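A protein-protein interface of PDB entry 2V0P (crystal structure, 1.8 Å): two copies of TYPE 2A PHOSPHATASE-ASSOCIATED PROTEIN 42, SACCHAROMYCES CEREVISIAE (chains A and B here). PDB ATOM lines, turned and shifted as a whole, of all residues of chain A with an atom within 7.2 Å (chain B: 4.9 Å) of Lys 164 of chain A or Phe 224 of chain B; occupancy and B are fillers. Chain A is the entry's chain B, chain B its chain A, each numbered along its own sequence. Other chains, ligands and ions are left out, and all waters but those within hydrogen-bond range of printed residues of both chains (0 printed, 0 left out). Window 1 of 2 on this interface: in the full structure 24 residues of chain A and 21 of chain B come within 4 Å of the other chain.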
ATOM      1  N   LYS A 154     -19.691 -24.614  13.953  1.00  0.00           N
ATOM      2  CA  LYS A 154     -18.882 -23.968  14.972  1.00  0.00           C
ATOM      3  C   LYS A 154     -19.414 -22.552  15.330  1.00  0.00           C
ATOM      4  O   LYS A 154     -19.656 -22.236  16.499  1.00  0.00           O
ATOM      5  CB  LYS A 154     -17.360 -23.916  14.602  1.00  0.00           C
ATOM      6  CG  LYS A 154     -16.517 -23.343  15.681  1.00  0.00           C
ATOM      7  CD  LYS A 154     -15.160 -22.879  15.184  1.00  0.00           C
ATOM      8  CE  LYS A 154     -14.157 -22.915  16.266  1.00  0.00           C
ATOM      9  NZ  LYS A 154     -12.816 -22.521  15.768  1.00  0.00           N
ATOM     10  N   LEU A 156     -22.451 -21.382  14.606  1.00  0.00           N
ATOM     11  CA  LEU A 156     -23.814 -21.498  15.125  1.00  0.00           C
ATOM     12  C   LEU A 156     -23.788 -21.778  16.622  1.00  0.00           C
ATOM     13  O   LEU A 156     -24.565 -21.176  17.374  1.00  0.00           O
ATOM     14  CB  LEU A 156     -24.572 -22.611  14.428  1.00  0.00           C
ATOM     15  CG  LEU A 156     -25.436 -22.272  13.219  1.00  0.00           C
ATOM     16  CD1 LEU A 156     -25.772 -23.544  12.492  1.00  0.00           C
ATOM     17  CD2 LEU A 156     -26.713 -21.583  13.674  1.00  0.00           C
ATOM     18  N   SER A 157     -22.904 -22.706  17.016  1.00  0.00           N
ATOM     19  CA  SER A 157     -22.773 -23.171  18.374  1.00  0.00           C
ATOM     20  C   SER A 157     -22.248 -22.020  19.212  1.00  0.00           C
ATOM     21  O   SER A 157     -22.748 -21.783  20.314  1.00  0.00           O
ATOM     22  CB  SER A 157     -21.778 -24.332  18.444  1.00  0.00           C
ATOM     23  OG  SER A 157     -22.431 -25.529  18.149  1.00  0.00           O
ATOM     24  N   GLY A 158     -21.327 -21.261  18.641  1.00  0.00           N
ATOM     25  CA  GLY A 158     -20.720 -20.096  19.270  1.00  0.00           C
ATOM     26  C   GLY A 158     -21.800 -19.047  19.542  1.00  0.00           C
ATOM     27  O   GLY A 158     -21.927 -18.555  20.632  1.00  0.00           O
ATOM     28  N   ALA A 159     -22.560 -18.736  18.509  1.00  0.00           N
ATOM     29  CA  ALA A 159     -23.685 -17.790  18.588  1.00  0.00           C
ATOM     30  C   ALA A 159     -24.768 -18.212  19.589  1.00  0.00           C
ATOM     31  O   ALA A 159     -25.300 -17.357  20.303  1.00  0.00           O
ATOM     32  CB  ALA A 159     -24.281 -17.601  17.218  1.00  0.00           C
ATOM     33  N   GLN A 160     -25.084 -19.505  19.650  1.00  0.00           N
ATOM     34  CA  GLN A 160     -26.038 -20.058  20.576  1.00  0.00           C
ATOM     35  C   GLN A 160     -25.587 -19.848  21.996  1.00  0.00           C
ATOM     36  O   GLN A 160     -26.337 -19.357  22.846  1.00  0.00           O
ATOM     37  CB  GLN A 160     -26.277 -21.548  20.296  1.00  0.00           C
ATOM     38  CG  GLN A 160     -27.223 -22.296  21.281  1.00  0.00           C
ATOM     39  CD  GLN A 160     -28.716 -22.033  21.095  1.00  0.00           C
ATOM     40  OE1 GLN A 160     -29.151 -20.917  20.802  1.00  0.00           O
ATOM     41  NE2 GLN A 160     -29.515 -23.076  21.292  1.00  0.00           N
ATOM     42  N   LEU A 161     -24.326 -20.193  22.226  1.00  0.00           N
ATOM     43  CA  LEU A 161     -23.741 -20.088  23.504  1.00  0.00           C
ATOM     44  C   LEU A 161     -23.928 -18.705  24.041  1.00  0.00           C
ATOM     45  O   LEU A 161     -24.248 -18.573  25.189  1.00  0.00           O
ATOM     46  CB  LEU A 161     -22.255 -20.429  23.399  1.00  0.00           C
ATOM     47  CG  LEU A 161     -21.541 -20.999  24.587  1.00  0.00           C
ATOM     48  CD1 LEU A 161     -22.368 -21.990  25.255  1.00  0.00           C
ATOM     49  CD2 LEU A 161     -20.199 -21.620  24.102  1.00  0.00           C
ATOM     50  N   LYS A 162     -23.692 -17.670  23.245  1.00  0.00           N
ATOM     51  CA  LYS A 162     -23.717 -16.278  23.738  1.00  0.00           C
ATOM     52  C   LYS A 162     -25.163 -15.825  23.963  1.00  0.00           C
ATOM     53  O   LYS A 162     -25.439 -15.080  24.919  1.00  0.00           O
ATOM     54  CB  LYS A 162     -23.098 -15.326  22.727  1.00  0.00           C
ATOM     55  CG  LYS A 162     -21.599 -15.254  22.730  1.00  0.00           C
ATOM     56  CD  LYS A 162     -21.104 -14.522  21.490  1.00  0.00           C
ATOM     57  CE  LYS A 162     -19.588 -14.394  21.484  1.00  0.00           C
ATOM     58  NZ  LYS A 162     -19.107 -13.370  22.462  1.00  0.00           N
ATOM     59  N   ARG A 163     -26.044 -16.218  23.062  1.00  0.00           N
ATOM     60  CA  ARG A 163     -27.477 -15.923  23.212  1.00  0.00           C
ATOM     61  C   ARG A 163     -28.040 -16.535  24.488  1.00  0.00           C
ATOM     62  O   ARG A 163     -28.787 -15.863  25.207  1.00  0.00           O
ATOM     63  CB  ARG A 163     -28.282 -16.354  21.985  1.00  0.00           C
ATOM     64  CG  ARG A 163     -28.038 -15.473  20.758  1.00  0.00           C
ATOM     65  CD  ARG A 163     -28.990 -15.843  19.608  1.00  0.00           C
ATOM     66  NE  ARG A 163     -28.257 -15.960  18.344  1.00  0.00           N
ATOM     67  CZ  ARG A 163     -28.077 -17.101  17.682  1.00  0.00           C
ATOM     68  NH1 ARG A 163     -28.586 -18.259  18.138  1.00  0.00           N
ATOM     69  NH2 ARG A 163     -27.393 -17.076  16.544  1.00  0.00           N
ATOM     70  N   LYS A 164     -27.645 -17.777  24.783  1.00  0.00           N
ATOM     71  CA  LYS A 164     -28.139 -18.541  25.931  1.00  0.00           C
ATOM     72  C   LYS A 164     -27.765 -17.979  27.296  1.00  0.00           C
ATOM     73  O   LYS A 164     -28.411 -18.337  28.293  1.00  0.00           O
ATOM     74  CB  LYS A 164     -27.788 -20.033  25.839  1.00  0.00           C
ATOM     75  CG  LYS A 164     -28.909 -20.902  25.221  1.00  0.00           C
ATOM     76  CD  LYS A 164     -28.469 -22.334  24.833  1.00  0.00           C
ATOM     77  CE  LYS A 164     -27.808 -23.113  25.997  1.00  0.00           C
ATOM     78  NZ  LYS A 164     -27.728 -24.584  25.664  1.00  0.00           N
ATOM     79  N   GLU A 165     -26.809 -17.049  27.319  1.00  0.00           N
ATOM     80  CA  GLU A 165     -26.306 -16.445  28.540  1.00  0.00           C
ATOM     81  C   GLU A 165     -26.641 -14.937  28.631  1.00  0.00           C
ATOM     82  O   GLU A 165     -26.345 -14.298  29.618  1.00  0.00           O
ATOM     83  CB  GLU A 165     -24.800 -16.721  28.706  1.00  0.00           C
ATOM     84  CG  GLU A 165     -23.865 -15.850  27.872  1.00  0.00           C
ATOM     85  CD  GLU A 165     -22.460 -16.436  27.744  1.00  0.00           C
ATOM     86  OE1 GLU A 165     -22.255 -17.649  28.021  1.00  0.00           O
ATOM     87  OE2 GLU A 165     -21.562 -15.683  27.337  1.00  0.00           O
ATOM     88  N   LYS A 166     -27.303 -14.397  27.601  1.00  0.00           N
ATOM     89  CA  LYS A 166     -27.850 -13.037  27.689  1.00  0.00           C
ATOM     90  C   LYS A 166     -28.761 -12.930  28.892  1.00  0.00           C
ATOM     91  O   LYS A 166     -29.507 -13.861  29.192  1.00  0.00           O
ATOM     92  CB  LYS A 166     -28.517 -12.574  26.383  1.00  0.00           C
ATOM     93  CG  LYS A 166     -27.443 -12.082  25.386  1.00  0.00           C
ATOM     94  CD  LYS A 166     -27.914 -10.986  24.429  1.00  0.00           C
ATOM     95  CE  LYS A 166     -26.720 -10.107  23.967  1.00  0.00           C
ATOM     96  NZ  LYS A 166     -26.474  -8.889  24.818  1.00  0.00           N
ATOM     97  N   ILE A 167     -28.634 -11.817  29.615  1.00  0.00           N
ATOM     98  CA  ILE A 167     -29.356 -11.577  30.869  1.00  0.00           C
ATOM     99  C   ILE A 167     -30.864 -11.305  30.677  1.00  0.00           C
ATOM    100  O   ILE A 167     -31.688 -11.862  31.388  1.00  0.00           O
ATOM    101  CB  ILE A 167     -28.682 -10.423  31.691  1.00  0.00           C
ATOM    102  CG1 ILE A 167     -27.255 -10.802  32.102  1.00  0.00           C
ATOM    103  CG2 ILE A 167     -29.523 -10.017  32.911  1.00  0.00           C
ATOM    104  CD1 ILE A 167     -27.132 -12.038  32.978  1.00  0.00           C
ATOM    105  N   LEU A 169     -33.347 -12.296  29.056  1.00  0.00           N
ATOM    106  CA  LEU A 169     -34.187 -13.498  29.117  1.00  0.00           C
ATOM    107  C   LEU A 169     -34.496 -13.938  30.537  1.00  0.00           C
ATOM    108  O   LEU A 169     -35.654 -14.194  30.868  1.00  0.00           O
ATOM    109  CB  LEU A 169     -33.439 -14.641  28.399  1.00  0.00           C
ATOM    110  CG  LEU A 169     -33.971 -16.071  28.163  1.00  0.00           C
ATOM    111  CD1 LEU A 169     -32.852 -16.961  27.601  1.00  0.00           C
ATOM    112  CD2 LEU A 169     -34.585 -16.745  29.399  1.00  0.00           C
ATOM    113  N   PHE A 170     -33.454 -14.053  31.361  1.00  0.00           N
ATOM    114  CA  PHE A 170     -33.562 -14.518  32.730  1.00  0.00           C
ATOM    115  C   PHE A 170     -34.226 -13.476  33.622  1.00  0.00           C
ATOM    116  O   PHE A 170     -34.982 -13.827  34.529  1.00  0.00           O
ATOM    117  CB  PHE A 170     -32.184 -14.802  33.304  1.00  0.00           C
ATOM    118  CG  PHE A 170     -31.473 -15.909  32.634  1.00  0.00           C
ATOM    119  CD1 PHE A 170     -31.593 -17.207  33.104  1.00  0.00           C
ATOM    120  CD2 PHE A 170     -30.651 -15.652  31.543  1.00  0.00           C
ATOM    121  CE1 PHE A 170     -30.912 -18.252  32.478  1.00  0.00           C
ATOM    122  CE2 PHE A 170     -29.955 -16.691  30.905  1.00  0.00           C
ATOM    123  CZ  PHE A 170     -30.090 -17.989  31.369  1.00  0.00           C
ATOM    124  N   ASN A 217     -38.116 -18.042  23.185  1.00  0.00           N
ATOM    125  CA  ASN A 217     -37.106 -18.984  23.608  1.00  0.00           C
ATOM    126  C   ASN A 217     -37.059 -20.257  22.748  1.00  0.00           C
ATOM    127  O   ASN A 217     -36.017 -20.571  22.144  1.00  0.00           O
ATOM    128  CB  ASN A 217     -37.366 -19.351  25.075  1.00  0.00           C
ATOM    129  CG  ASN A 217     -36.304 -20.280  25.651  1.00  0.00           C
ATOM    130  OD1 ASN A 217     -36.121 -21.412  25.183  1.00  0.00           O
ATOM    131  ND2 ASN A 217     -35.599 -19.803  26.689  1.00  0.00           N
ATOM    132  N   GLU A 220     -36.112 -19.835  18.943  1.00  0.00           N
ATOM    133  CA  GLU A 220     -34.664 -19.721  18.816  1.00  0.00           C
ATOM    134  C   GLU A 220     -33.963 -21.077  18.948  1.00  0.00           C
ATOM    135  O   GLU A 220     -33.193 -21.425  18.110  1.00  0.00           O
ATOM    136  CB  GLU A 220     -34.098 -18.676  19.795  1.00  0.00           C
ATOM    137  CG  GLU A 220     -34.555 -17.252  19.463  1.00  0.00           C
ATOM    138  CD  GLU A 220     -33.578 -16.171  19.894  1.00  0.00           C
ATOM    139  OE1 GLU A 220     -33.464 -15.899  21.117  1.00  0.00           O
ATOM    140  OE2 GLU A 220     -32.939 -15.572  18.995  1.00  0.00           O
ATOM    141  N   GLN A 221     -34.254 -21.833  19.990  1.00  0.00           N
ATOM    142  CA  GLN A 221     -33.677 -23.148  20.165  1.00  0.00           C
ATOM    143  C   GLN A 221     -33.915 -24.048  18.959  1.00  0.00           C
ATOM    144  O   GLN A 221     -33.031 -24.695  18.499  1.00  0.00           O
ATOM    145  CB  GLN A 221     -34.215 -23.802  21.431  1.00  0.00           C
ATOM    146  CG  GLN A 221     -33.590 -25.121  21.788  1.00  0.00           C
ATOM    147  CD  GLN A 221     -32.103 -24.994  22.130  1.00  0.00           C
ATOM    148  OE1 GLN A 221     -31.665 -23.979  22.674  1.00  0.00           O
ATOM    149  NE2 GLN A 221     -31.328 -26.029  21.804  1.00  0.00           N
ATOM    150  N   PHE A 224     -32.024 -22.734  15.784  1.00  0.00           N
ATOM    151  CA  PHE A 224     -30.608 -23.141  15.951  1.00  0.00           C
ATOM    152  C   PHE A 224     -30.451 -24.616  15.579  1.00  0.00           C
ATOM    153  O   PHE A 224     -29.672 -24.952  14.683  1.00  0.00           O
ATOM    154  CB  PHE A 224     -30.154 -22.872  17.388  1.00  0.00           C
ATOM    155  CG  PHE A 224     -29.002 -23.727  17.840  1.00  0.00           C
ATOM    156  CD1 PHE A 224     -27.692 -23.486  17.371  1.00  0.00           C
ATOM    157  CD2 PHE A 224     -29.211 -24.761  18.736  1.00  0.00           C
ATOM    158  CE1 PHE A 224     -26.657 -24.275  17.769  1.00  0.00           C
ATOM    159  CE2 PHE A 224     -28.140 -25.551  19.168  1.00  0.00           C
ATOM    160  CZ  PHE A 224     -26.870 -25.310  18.671  1.00  0.00           C
ATOM    161  N   MET A 228     -28.492 -26.299  12.312  1.00  0.00           N
ATOM    162  CA  MET A 228     -27.433 -27.248  12.546  1.00  0.00           C
ATOM    163  C   MET A 228     -27.666 -28.482  11.721  1.00  0.00           C
ATOM    164  O   MET A 228     -26.761 -28.972  11.030  1.00  0.00           O
ATOM    165  CB  MET A 228     -27.388 -27.604  14.030  1.00  0.00           C
ATOM    166  CG  MET A 228     -26.455 -28.706  14.389  1.00  0.00           C
ATOM    167  SD  MET A 228     -25.624 -28.234  16.071  1.00  0.00           S
ATOM    168  CE  MET A 228     -25.296 -26.338  15.644  1.00  0.00           C
ATOM    169  N   LEU B 143     -18.474 -28.726  30.852  1.00  0.00           N
ATOM    170  CA  LEU B 143     -18.779 -27.310  30.671  1.00  0.00           C
ATOM    171  C   LEU B 143     -19.439 -26.738  31.910  1.00  0.00           C
ATOM    172  O   LEU B 143     -19.343 -25.545  32.195  1.00  0.00           O
ATOM    173  CB  LEU B 143     -19.660 -27.148  29.425  1.00  0.00           C
ATOM    174  CG  LEU B 143     -19.917 -25.820  28.734  1.00  0.00           C
ATOM    175  CD1 LEU B 143     -18.687 -25.177  28.283  1.00  0.00           C
ATOM    176  CD2 LEU B 143     -20.817 -26.112  27.530  1.00  0.00           C
ATOM    177  N   GLU B 220     -14.243 -24.188  25.980  1.00  0.00           N
ATOM    178  CA  GLU B 220     -15.739 -23.924  26.146  1.00  0.00           C
ATOM    179  C   GLU B 220     -16.480 -24.204  24.832  1.00  0.00           C
ATOM    180  O   GLU B 220     -17.518 -24.949  24.803  1.00  0.00           O
ATOM    181  CB  GLU B 220     -15.975 -22.483  26.622  1.00  0.00           C
ATOM    182  CG  GLU B 220     -17.368 -22.256  27.208  1.00  0.00           C
ATOM    183  CD  GLU B 220     -17.802 -20.806  27.216  1.00  0.00           C
ATOM    184  OE1 GLU B 220     -17.122 -19.926  26.644  1.00  0.00           O
ATOM    185  OE2 GLU B 220     -18.856 -20.548  27.785  1.00  0.00           O
ATOM    186  N   GLN B 221     -15.947 -23.658  23.751  1.00  0.00           N
ATOM    187  CA  GLN B 221     -16.547 -23.751  22.451  1.00  0.00           C
ATOM    188  C   GLN B 221     -16.578 -25.211  22.050  1.00  0.00           C
ATOM    189  O   GLN B 221     -17.584 -25.658  21.630  1.00  0.00           O
ATOM    190  CB  GLN B 221     -15.796 -22.940  21.435  1.00  0.00           C
ATOM    191  CG  GLN B 221     -16.051 -23.331  20.017  1.00  0.00           C
ATOM    192  CD  GLN B 221     -17.475 -22.981  19.553  1.00  0.00           C
ATOM    193  OE1 GLN B 221     -18.041 -21.969  19.957  1.00  0.00           O
ATOM    194  NE2 GLN B 221     -18.036 -23.813  18.699  1.00  0.00           N
ATOM    195  N   ASN B 222     -15.495 -25.956  22.268  1.00  0.00           N
ATOM    196  CA  ASN B 222     -15.500 -27.351  21.859  1.00  0.00           C
ATOM    197  C   ASN B 222     -16.418 -28.264  22.704  1.00  0.00           C
ATOM    198  O   ASN B 222     -16.989 -29.201  22.213  1.00  0.00           O
ATOM    199  CB  ASN B 222     -14.041 -27.884  21.771  1.00  0.00           C
ATOM    200  CG  ASN B 222     -13.226 -27.220  20.673  1.00  0.00           C
ATOM    201  OD1 ASN B 222     -13.716 -26.419  19.906  1.00  0.00           O
ATOM    202  ND2 ASN B 222     -11.964 -27.519  20.635  1.00  0.00           N
ATOM    203  N   LEU B 223     -16.537 -27.998  23.985  1.00  0.00           N
ATOM    204  CA  LEU B 223     -17.365 -28.762  24.822  1.00  0.00           C
ATOM    205  C   LEU B 223     -18.838 -28.495  24.444  1.00  0.00           C
ATOM    206  O   LEU B 223     -19.545 -29.400  24.254  1.00  0.00           O
ATOM    207  CB  LEU B 223     -17.115 -28.391  26.280  1.00  0.00           C
ATOM    208  CG  LEU B 223     -15.807 -28.984  26.830  1.00  0.00           C
ATOM    209  CD1 LEU B 223     -15.723 -28.713  28.339  1.00  0.00           C
ATOM    210  CD2 LEU B 223     -15.751 -30.452  26.565  1.00  0.00           C
ATOM    211  N   PHE B 224     -19.194 -27.250  24.244  1.00  0.00           N
ATOM    212  CA  PHE B 224     -20.556 -26.887  23.841  1.00  0.00           C
ATOM    213  C   PHE B 224     -20.908 -27.455  22.480  1.00  0.00           C
ATOM    214  O   PHE B 224     -21.968 -28.075  22.322  1.00  0.00           O
ATOM    215  CB  PHE B 224     -20.690 -25.401  23.769  1.00  0.00           C
ATOM    216  CG  PHE B 224     -22.113 -24.979  23.598  1.00  0.00           C
ATOM    217  CD1 PHE B 224     -22.999 -25.138  24.639  1.00  0.00           C
ATOM    218  CD2 PHE B 224     -22.570 -24.494  22.385  1.00  0.00           C
ATOM    219  CE1 PHE B 224     -24.355 -24.734  24.500  1.00  0.00           C
ATOM    220  CE2 PHE B 224     -23.929 -24.113  22.235  1.00  0.00           C
ATOM    221  CZ  PHE B 224     -24.783 -24.219  23.295  1.00  0.00           C
ATOM    222  N   GLU B 225     -20.012 -27.240  21.504  1.00  0.00           N
ATOM    223  CA  GLU B 225     -20.158 -27.755  20.162  1.00  0.00           C
ATOM    224  C   GLU B 225     -20.291 -29.258  20.207  1.00  0.00           C
ATOM    225  O   GLU B 225     -21.241 -29.802  19.607  1.00  0.00           O
ATOM    226  CB  GLU B 225     -19.002 -27.328  19.274  1.00  0.00           C
ATOM    227  CG  GLU B 225     -19.219 -27.484  17.763  1.00  0.00           C
ATOM    228  CD  GLU B 225     -17.962 -27.105  16.993  1.00  0.00           C
ATOM    229  OE1 GLU B 225     -17.350 -26.066  17.325  1.00  0.00           O
ATOM    230  OE2 GLU B 225     -17.568 -27.842  16.055  1.00  0.00           O
ATOM    231  N   CYS B 226     -19.422 -29.936  20.967  1.00  0.00           N
ATOM    232  CA  CYS B 226     -19.549 -31.385  21.108  1.00  0.00           C
ATOM    233  C   CYS B 226     -20.913 -31.878  21.658  1.00  0.00           C
ATOM    234  O   CYS B 226     -21.546 -32.790  21.123  1.00  0.00           O
ATOM    235  CB  CYS B 226     -18.458 -31.922  21.989  1.00  0.00           C
ATOM    236  SG  CYS B 226     -18.408 -33.707  21.925  1.00  0.00           S
ATOM    237  N   GLU B 227     -21.331 -31.291  22.761  1.00  0.00           N
ATOM    238  CA  GLU B 227     -22.605 -31.623  23.331  1.00  0.00           C
ATOM    239  C   GLU B 227     -23.767 -31.386  22.344  1.00  0.00           C
ATOM    240  O   GLU B 227     -24.681 -32.209  22.245  1.00  0.00           O
ATOM    241  CB  GLU B 227     -22.803 -30.847  24.598  1.00  0.00           C
ATOM    242  CG  GLU B 227     -21.912 -31.293  25.732  1.00  0.00           C
ATOM    243  CD  GLU B 227     -22.039 -30.392  26.961  1.00  0.00           C
ATOM    244  OE1 GLU B 227     -23.180 -30.048  27.358  1.00  0.00           O
ATOM    245  OE2 GLU B 227     -20.982 -30.027  27.525  1.00  0.00           O
ATOM    246  N   MET B 228     -23.702 -30.311  21.573  1.00  0.00           N
ATOM    247  CA  MET B 228     -24.765 -29.995  20.628  1.00  0.00           C
ATOM    248  C   MET B 228     -24.843 -31.021  19.498  1.00  0.00           C
ATOM    249  O   MET B 228     -25.907 -31.526  19.240  1.00  0.00           O
ATOM    250  CB  MET B 228     -24.659 -28.557  20.093  1.00  0.00           C
ATOM    251  CG  MET B 228     -24.721 -27.547  21.182  1.00  0.00           C
ATOM    252  SD  MET B 228     -26.556 -27.366  21.850  1.00  0.00           S
ATOM    253  CE  MET B 228     -26.533 -28.407  23.515  1.00  0.00           C
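The backbone carbonyl oxygen (O) of Lys 154 of chain A lies within hydrogen-bond range of the side-chain amide nitrogen (NE2) of Gln 221 of chain B (3.2 Å).
NE2 of Gln 160 of chain A sits at hydrogen-bond distance from OE1 of Gln 221 of chain A, 2.7 Å away.
NE2 of Gln 221 of chain B sits at hydrogen-bond distance from OE1 of Glu 225 of chain B.
Glu 225 of chain B touches Lys 154 of chain A (OE1 to CG, 3.3 Å).
Ser 157 of chain A touches Gln 221 of chain B (CB to NE2, 3.8 Å).
Ser 157 of chain A touches Phe 224 of chain B.
OG of Ser 157 of chain A touches CA of Glu 225 of chain B, at 3.8 Å.
OE1 of Gln 221 of chain B touches CA of Gly 158 of chain A (3.3 Å).
Phe 224 of chain B touches Gln 160 of chain A.
CD1 of Leu 161 of chain A touches CD1 of Phe 224 of chain B, at 3.3 Å.
CE1 of Phe 224 of chain B touches NZ of Lys 164 of chain A, at 3.6 Å.
CE2 of Phe 224 of chain A touches SD of Met 228 of chain B, 3.6 Å away.
Leu 156 of chain A touches none of the printed residues of chain B.
Of the printed residues of chain B, Gly 158 of chain A touches Gln 221.
Of the printed residues of chain B, Leu 161 of chain A touches Phe 224 (3.3 Å).
Lys 164 of chain A touches just one residue of chain B: Phe 224.
Of the printed residues of chain B, Phe 224 of chain A touches Met 228 (3.6 Å).
Glu 220 of chain B touches none of the printed residues of chain A.
Phe 224 of chain B touches just these residues of chain A: Ser 157 (3.2 Å), Gln 160 (3.7 Å), Leu 161 (3.3 Å) and Lys 164 (3.6 Å).
Printed residues of chain A within 4 Å of Met 228 of chain B: Phe 224 (3.6 Å).
The nearest printed residue of chain B that does not touch Ser 157 of chain A is Met 228 of chain B (4.2 Å).
Of the 10 printed residues of chain B, 4 touch a printed residue of chain A.
Hydrophobic or aromatic side chains of chain B that line the printed part of chain A: Phe 224 and Met 228.
Printed residues of chain A that touch a printed residue of chain B: Lys 154, Ser 157, Gly 158, Gln 160, Leu 161, Lys 164 and Phe 224.
Among the printed residues, 10 pairs touch across the chains.
Phe 224 of chain A touches Met 228 of chain B, but with the chains exchanged Met 228 of chain A does not touch Phe 224 of chain B (7.1 Å).
Positions printed for both chains: 220, 221, 224 and 228.
Of the 10 pairs that touch across the chains among the printed residues, none has its exchanged pair printed and touching as well.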
